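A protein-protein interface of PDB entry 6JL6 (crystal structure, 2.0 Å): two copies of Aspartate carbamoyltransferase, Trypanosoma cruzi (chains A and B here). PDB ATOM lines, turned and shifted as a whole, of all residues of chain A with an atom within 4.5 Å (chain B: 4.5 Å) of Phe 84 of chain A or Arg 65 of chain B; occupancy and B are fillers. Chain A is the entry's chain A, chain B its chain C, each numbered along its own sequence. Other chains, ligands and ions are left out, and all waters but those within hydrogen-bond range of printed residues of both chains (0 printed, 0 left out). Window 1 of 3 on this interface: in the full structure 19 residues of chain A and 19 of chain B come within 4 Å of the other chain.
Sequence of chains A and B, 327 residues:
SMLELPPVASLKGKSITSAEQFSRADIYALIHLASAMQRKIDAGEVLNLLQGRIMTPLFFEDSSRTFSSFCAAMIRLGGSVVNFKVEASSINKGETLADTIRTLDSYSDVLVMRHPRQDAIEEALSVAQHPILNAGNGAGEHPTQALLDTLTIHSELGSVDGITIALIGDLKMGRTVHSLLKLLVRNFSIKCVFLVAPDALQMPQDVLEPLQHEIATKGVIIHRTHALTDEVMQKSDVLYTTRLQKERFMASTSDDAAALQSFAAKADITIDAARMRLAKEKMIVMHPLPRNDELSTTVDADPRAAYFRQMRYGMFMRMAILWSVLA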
ATOM      1  N   THR A  56       7.853 -24.782  -2.845  1.00  0.00           N
ATOM      2  CA  THR A  56       8.075 -25.771  -3.874  1.00  0.00           C
ATOM      3  C   THR A  56       9.565 -26.114  -3.929  1.00  0.00           C
ATOM      4  O   THR A  56      10.382 -25.242  -4.183  1.00  0.00           O
ATOM      5  CB  THR A  56       7.590 -25.307  -5.249  1.00  0.00           C
ATOM      6  OG1 THR A  56       6.205 -24.953  -5.168  1.00  0.00           O
ATOM      7  CG2 THR A  56       7.766 -26.448  -6.265  1.00  0.00           C
ATOM      8  N   PRO A  57       9.914 -27.389  -3.670  1.00  0.00           N
ATOM      9  CA  PRO A  57      11.250 -27.916  -3.900  1.00  0.00           C
ATOM     10  C   PRO A  57      11.586 -28.036  -5.383  1.00  0.00           C
ATOM     11  O   PRO A  57      10.721 -28.379  -6.205  1.00  0.00           O
ATOM     12  CB  PRO A  57      11.193 -29.323  -3.270  1.00  0.00           C
ATOM     13  CG  PRO A  57      10.023 -29.296  -2.372  1.00  0.00           C
ATOM     14  CD  PRO A  57       9.050 -28.423  -3.085  1.00  0.00           C
ATOM     15  N   LEU A  58      12.835 -27.732  -5.713  1.00  0.00           N
ATOM     16  CA  LEU A  58      13.347 -27.873  -7.049  1.00  0.00           C
ATOM     17  C   LEU A  58      14.704 -28.545  -6.933  1.00  0.00           C
ATOM     18  O   LEU A  58      15.748 -27.881  -6.894  1.00  0.00           O
ATOM     19  CB  LEU A  58      13.431 -26.508  -7.716  1.00  0.00           C
ATOM     20  CG  LEU A  58      13.904 -26.543  -9.163  1.00  0.00           C
ATOM     21  CD1 LEU A  58      13.045 -27.462 -10.030  1.00  0.00           C
ATOM     22  CD2 LEU A  58      13.922 -25.132  -9.705  1.00  0.00           C
ATOM     23  N   VAL A  82       4.223 -28.045  -2.612  1.00  0.00           N
ATOM     24  CA  VAL A  82       3.850 -28.640  -3.893  1.00  0.00           C
ATOM     25  C   VAL A  82       5.002 -29.521  -4.306  1.00  0.00           C
ATOM     26  O   VAL A  82       6.119 -29.040  -4.534  1.00  0.00           O
ATOM     27  CB  VAL A  82       3.505 -27.584  -4.958  1.00  0.00           C
ATOM     28  CG1 VAL A  82       3.478 -28.191  -6.352  1.00  0.00           C
ATOM     29  CG2 VAL A  82       2.158 -26.958  -4.626  1.00  0.00           C
ATOM     30  N   ASN A  83       4.701 -30.806  -4.422  1.00  0.00           N
ATOM     31  CA  ASN A  83       5.703 -31.848  -4.629  1.00  0.00           C
ATOM     32  C   ASN A  83       6.232 -31.945  -6.065  1.00  0.00           C
ATOM     33  O   ASN A  83       6.031 -32.964  -6.729  1.00  0.00           O
ATOM     34  CB  ASN A  83       5.127 -33.209  -4.188  1.00  0.00           C
ATOM     35  CG  ASN A  83       5.825 -33.748  -2.980  1.00  0.00           C
ATOM     36  OD1 ASN A  83       6.746 -34.570  -3.094  1.00  0.00           O
ATOM     37  ND2 ASN A  83       5.430 -33.259  -1.810  1.00  0.00           N
ATOM     38  N   PHE A  84       6.912 -30.905  -6.543  1.00  0.00           N
ATOM     39  CA  PHE A  84       7.478 -30.930  -7.887  1.00  0.00           C
ATOM     40  C   PHE A  84       8.690 -31.882  -7.988  1.00  0.00           C
ATOM     41  O   PHE A  84       9.531 -31.918  -7.083  1.00  0.00           O
ATOM     42  CB  PHE A  84       7.890 -29.524  -8.320  1.00  0.00           C
ATOM     43  CG  PHE A  84       8.437 -29.470  -9.708  1.00  0.00           C
ATOM     44  CD1 PHE A  84       7.604 -29.694 -10.800  1.00  0.00           C
ATOM     45  CD2 PHE A  84       9.781 -29.224  -9.937  1.00  0.00           C
ATOM     46  CE1 PHE A  84       8.102 -29.673 -12.092  1.00  0.00           C
ATOM     47  CE2 PHE A  84      10.283 -29.190 -11.236  1.00  0.00           C
ATOM     48  CZ  PHE A  84       9.445 -29.417 -12.312  1.00  0.00           C
ATOM     49  N   LYS A  85       8.766 -32.646  -9.079  1.00  0.00           N
ATOM     50  CA  LYS A  85       9.897 -33.557  -9.352  1.00  0.00           C
ATOM     51  C   LYS A  85      10.504 -33.214 -10.690  1.00  0.00           C
ATOM     52  O   LYS A  85       9.782 -32.967 -11.646  1.00  0.00           O
ATOM     53  CB  LYS A  85       9.466 -35.021  -9.410  1.00  0.00           C
ATOM     54  CG  LYS A  85       9.098 -35.641  -8.073  1.00  0.00           C
ATOM     55  CD  LYS A  85       7.588 -35.680  -7.857  1.00  0.00           C
ATOM     56  CE  LYS A  85       7.228 -36.085  -6.432  1.00  0.00           C
ATOM     57  NZ  LYS A  85       7.855 -37.378  -6.037  1.00  0.00           N
ATOM     58  N   VAL A  86      11.833 -33.231 -10.754  1.00  0.00           N
ATOM     59  CA  VAL A  86      12.558 -33.022 -12.008  1.00  0.00           C
ATOM     60  C   VAL A  86      12.435 -34.268 -12.890  1.00  0.00           C
ATOM     61  O   VAL A  86      12.050 -34.160 -14.045  1.00  0.00           O
ATOM     62  CB  VAL A  86      14.034 -32.628 -11.758  1.00  0.00           C
ATOM     63  CG1 VAL A  86      14.884 -32.766 -13.017  1.00  0.00           C
ATOM     64  CG2 VAL A  86      14.099 -31.203 -11.234  1.00  0.00           C
ATOM     65  N   GLU A  95      12.818 -28.338 -21.699  1.00  0.00           N
ATOM     66  CA  GLU A  95      12.578 -27.063 -20.995  1.00  0.00           C
ATOM     67  C   GLU A  95      13.844 -26.603 -20.257  1.00  0.00           C
ATOM     68  O   GLU A  95      14.500 -27.409 -19.632  1.00  0.00           O
ATOM     69  CB  GLU A  95      11.419 -27.198 -19.998  1.00  0.00           C
ATOM     70  CG  GLU A  95      11.155 -25.926 -19.201  1.00  0.00           C
ATOM     71  CD  GLU A  95       9.734 -25.841 -18.688  1.00  0.00           C
ATOM     72  OE1 GLU A  95       9.255 -26.849 -18.124  1.00  0.00           O
ATOM     73  OE2 GLU A  95       9.083 -24.778 -18.857  1.00  0.00           O
ATOM     74  N   THR A 100      11.723 -23.440 -16.104  1.00  0.00           N
ATOM     75  CA  THR A 100      11.309 -24.241 -14.939  1.00  0.00           C
ATOM     76  C   THR A 100      11.131 -23.348 -13.718  1.00  0.00           C
ATOM     77  O   THR A 100      10.122 -23.452 -13.021  1.00  0.00           O
ATOM     78  CB  THR A 100      12.314 -25.364 -14.610  1.00  0.00           C
ATOM     79  OG1 THR A 100      12.491 -26.183 -15.767  1.00  0.00           O
ATOM     80  CG2 THR A 100      11.798 -26.244 -13.446  1.00  0.00           C
ATOM     81  N   THR A 103       8.037 -21.210 -14.139  1.00  0.00           N
ATOM     82  CA  THR A 103       6.878 -22.068 -13.914  1.00  0.00           C
ATOM     83  C   THR A 103       6.542 -22.206 -12.415  1.00  0.00           C
ATOM     84  O   THR A 103       5.416 -21.894 -11.973  1.00  0.00           O
ATOM     85  CB  THR A 103       7.083 -23.463 -14.553  1.00  0.00           C
ATOM     86  OG1 THR A 103       7.400 -23.309 -15.943  1.00  0.00           O
ATOM     87  CG2 THR A 103       5.850 -24.330 -14.412  1.00  0.00           C
ATOM     88  N   LEU A 104       7.522 -22.639 -11.637  1.00  0.00           N
ATOM     89  CA  LEU A 104       7.339 -22.802 -10.179  1.00  0.00           C
ATOM     90  C   LEU A 104       6.995 -21.451  -9.513  1.00  0.00           C
ATOM     91  O   LEU A 104       6.124 -21.373  -8.641  1.00  0.00           O
ATOM     92  CB  LEU A 104       8.572 -23.462  -9.538  1.00  0.00           C
ATOM     93  CG  LEU A 104       8.763 -24.976  -9.742  1.00  0.00           C
ATOM     94  CD1 LEU A 104       7.506 -25.698  -9.363  1.00  0.00           C
ATOM     95  CD2 LEU A 104       9.106 -25.455 -11.146  1.00  0.00           C
ATOM     96  N   SER B  63       4.153 -35.641 -16.169  1.00  0.00           N
ATOM     97  CA  SER B  63       4.491 -34.249 -16.299  1.00  0.00           C
ATOM     98  C   SER B  63       4.234 -33.731 -14.894  1.00  0.00           C
ATOM     99  O   SER B  63       3.117 -33.301 -14.571  1.00  0.00           O
ATOM    100  CB  SER B  63       3.588 -33.554 -17.326  1.00  0.00           C
ATOM    101  OG  SER B  63       3.645 -32.142 -17.211  1.00  0.00           O
ATOM    102  N   SER B  64       5.247 -33.848 -14.036  1.00  0.00           N
ATOM    103  CA  SER B  64       5.187 -33.232 -12.703  1.00  0.00           C
ATOM    104  C   SER B  64       4.900 -31.722 -12.839  1.00  0.00           C
ATOM    105  O   SER B  64       4.285 -31.120 -11.951  1.00  0.00           O
ATOM    106  CB  SER B  64       6.476 -33.501 -11.905  1.00  0.00           C
ATOM    107  OG  SER B  64       6.364 -33.050 -10.561  1.00  0.00           O
ATOM    108  N   ARG B  65       5.318 -31.139 -13.966  1.00  0.00           N
ATOM    109  CA  ARG B  65       4.982 -29.765 -14.336  1.00  0.00           C
ATOM    110  C   ARG B  65       3.466 -29.454 -14.282  1.00  0.00           C
ATOM    111  O   ARG B  65       3.058 -28.488 -13.626  1.00  0.00           O
ATOM    112  CB  ARG B  65       5.508 -29.481 -15.747  1.00  0.00           C
ATOM    113  CG  ARG B  65       5.333 -28.047 -16.192  1.00  0.00           C
ATOM    114  CD  ARG B  65       5.405 -27.882 -17.708  1.00  0.00           C
ATOM    115  NE  ARG B  65       5.018 -26.514 -18.065  1.00  0.00           N
ATOM    116  CZ  ARG B  65       5.784 -25.435 -17.897  1.00  0.00           C
ATOM    117  NH1 ARG B  65       5.327 -24.237 -18.215  1.00  0.00           N
ATOM    118  NH2 ARG B  65       7.008 -25.532 -17.400  1.00  0.00           N
ATOM    119  N   THR B  66       2.647 -30.243 -14.988  1.00  0.00           N
ATOM    120  CA  THR B  66       1.210 -29.940 -15.084  1.00  0.00           C
ATOM    121  C   THR B  66       0.477 -30.306 -13.787  1.00  0.00           C
ATOM    122  O   THR B  66      -0.379 -29.535 -13.327  1.00  0.00           O
ATOM    123  CB  THR B  66       0.553 -30.598 -16.315  1.00  0.00           C
ATOM    124  OG1 THR B  66       1.193 -30.115 -17.503  1.00  0.00           O
ATOM    125  CG2 THR B  66      -0.950 -30.243 -16.397  1.00  0.00           C
ATOM    126  N   PHE B  67       0.836 -31.451 -13.202  1.00  0.00           N
ATOM    127  CA  PHE B  67       0.228 -31.881 -11.953  1.00  0.00           C
ATOM    128  C   PHE B  67       0.486 -30.879 -10.829  1.00  0.00           C
ATOM    129  O   PHE B  67      -0.382 -30.675  -9.998  1.00  0.00           O
ATOM    130  CB  PHE B  67       0.620 -33.320 -11.514  1.00  0.00           C
ATOM    131  CG  PHE B  67      -0.245 -33.856 -10.384  1.00  0.00           C
ATOM    132  CD1 PHE B  67      -1.647 -33.860 -10.494  1.00  0.00           C
ATOM    133  CD2 PHE B  67       0.318 -34.300  -9.192  1.00  0.00           C
ATOM    134  CE1 PHE B  67      -2.459 -34.323  -9.452  1.00  0.00           C
ATOM    135  CE2 PHE B  67      -0.497 -34.770  -8.147  1.00  0.00           C
ATOM    136  CZ  PHE B  67      -1.881 -34.774  -8.275  1.00  0.00           C
ATOM    137  N   SER B  68       1.652 -30.235 -10.842  1.00  0.00           N
ATOM    138  CA  SER B  68       2.019 -29.262  -9.816  1.00  0.00           C
ATOM    139  C   SER B  68       1.209 -27.961  -9.897  1.00  0.00           C
ATOM    140  O   SER B  68       0.860 -27.387  -8.865  1.00  0.00           O
ATOM    141  CB  SER B  68       3.534 -28.992  -9.847  1.00  0.00           C
ATOM    142  OG  SER B  68       4.212 -30.162  -9.406  1.00  0.00           O
ATOM    143  N   SER B  69       0.882 -27.518 -11.109  1.00  0.00           N
ATOM    144  CA  SER B  69      -0.044 -26.397 -11.279  1.00  0.00           C
ATOM    145  C   SER B  69      -1.466 -26.695 -10.735  1.00  0.00           C
ATOM    146  O   SER B  69      -2.108 -25.813 -10.153  1.00  0.00           O
ATOM    147  CB  SER B  69      -0.122 -25.977 -12.752  1.00  0.00           C
ATOM    148  OG  SER B  69      -0.831 -26.935 -13.508  1.00  0.00           O
ATOM    149  N   LEU B 289       3.314 -23.865 -23.106  1.00  0.00           N
ATOM    150  CA  LEU B 289       4.600 -24.203 -22.499  1.00  0.00           C
ATOM    151  C   LEU B 289       4.592 -25.710 -22.191  1.00  0.00           C
ATOM    152  O   LEU B 289       3.515 -26.300 -22.081  1.00  0.00           O
ATOM    153  CB  LEU B 289       4.988 -23.329 -21.280  1.00  0.00           C
ATOM    154  CG  LEU B 289       5.300 -21.858 -21.569  1.00  0.00           C
ATOM    155  CD1 LEU B 289       5.595 -21.138 -20.268  1.00  0.00           C
ATOM    156  CD2 LEU B 289       6.445 -21.656 -22.551  1.00  0.00           C
ATOM    157  N   PRO B 290       5.750 -26.357 -22.115  1.00  0.00           N
ATOM    158  CA  PRO B 290       7.062 -25.759 -22.320  1.00  0.00           C
ATOM    159  C   PRO B 290       7.377 -25.508 -23.784  1.00  0.00           C
ATOM    160  O   PRO B 290       6.745 -26.087 -24.665  1.00  0.00           O
ATOM    161  CB  PRO B 290       8.010 -26.835 -21.786  1.00  0.00           C
ATOM    162  CG  PRO B 290       7.307 -28.102 -22.111  1.00  0.00           C
ATOM    163  CD  PRO B 290       5.851 -27.803 -21.853  1.00  0.00           C
ATOM    164  N   MET B 311       0.670 -18.569 -17.224  1.00  0.00           N
ATOM    165  CA  MET B 311       0.729 -19.632 -16.194  1.00  0.00           C
ATOM    166  C   MET B 311       0.070 -19.207 -14.875  1.00  0.00           C
ATOM    167  O   MET B 311      -0.571 -20.029 -14.211  1.00  0.00           O
ATOM    168  CB  MET B 311       2.172 -20.081 -15.952  1.00  0.00           C
ATOM    169  CG  MET B 311       2.777 -20.815 -17.135  1.00  0.00           C
ATOM    170  SD  MET B 311       4.371 -21.564 -16.731  1.00  0.00           S
ATOM    171  CE  MET B 311       5.343 -20.057 -16.699  1.00  0.00           C
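The side-chain carboxylate (OE2) of Glu 95 of chain A lies within salt-bridge range of the guanidinium group (NH2) of Arg 65 of chain B (2.6 Å). The backbone NH (N) of Lys 85 of chain A is in hydrogen-bond range of the side-chain hydroxyl (OG) of Ser 64 of chain B. OG1 of Thr 103 of chain A lies within hydrogen-bond range of SD of Met 311 of chain B. NH2 of Arg 65 of chain B sits at hydrogen-bond distance from OG1 of Thr 103 of chain A.
The backbone carbonyl oxygen of Ser 64 of chain B sits at hydrogen-bond distance from the side-chain hydroxyl of Ser 68 of chain B, 2.7 Å away. NH1 of Arg 65 of chain B lies within hydrogen-bond range of SD of Met 311 of chain B, 3.2 Å away.
Among the printed residues, merely in contact across the chains: Val 82 of chain A with Ser 68 of chain B, Asn 83 of chain A with Ser 64 of chain B, Phe 84 of chain A with Ser 64 of chain B, Phe 84 of chain A with Arg 65 of chain B, Phe 84 of chain A with Ser 68 of chain B and Glu 95 of chain A with Pro 290 of chain B.
Pro 57 of chain A touches none of the printed residues of chain B. Phe 84 of chain A touches just these residues of chain B: Ser 64, Arg 65 and Ser 68. Of the printed residues of chain B, Lys 85 of chain A touches Ser 64. Of the printed residues of chain B, Thr 103 of chain A touches Arg 65 and Met 311. Ser 63 of chain B touches none of the printed residues of chain A. Of chain A, only Phe 84, Glu 95 and Thr 103 come within 4 Å of Arg 65 of chain B. The nearest printed residue of chain A that does not touch Arg 65 of chain B is Thr 100 of chain A (5.1 Å). The nearest printed residue of chain B that does not touch Thr 103 of chain A is Leu 289 of chain B (5.2 Å).
Of the 10 printed residues of chain B, 5 touch a printed residue of chain A. Printed residues of chain B that touch a printed residue of chain A: Ser 64, Arg 65, Ser 68, Pro 290 and Met 311. Hydrophobic or aromatic side chains of chain B within 4 Å of the printed part of chain A: Pro 290 and Met 311. Among the printed residues, 10 pairs touch across the chains. Among the printed residues, Asp or Glu carboxylates within 4 Å of a Lys or Arg side-chain nitrogen of the other chain: Glu 95 of chain A with Arg 65 of chain B (2.6 Å).
No position is printed for both chains.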
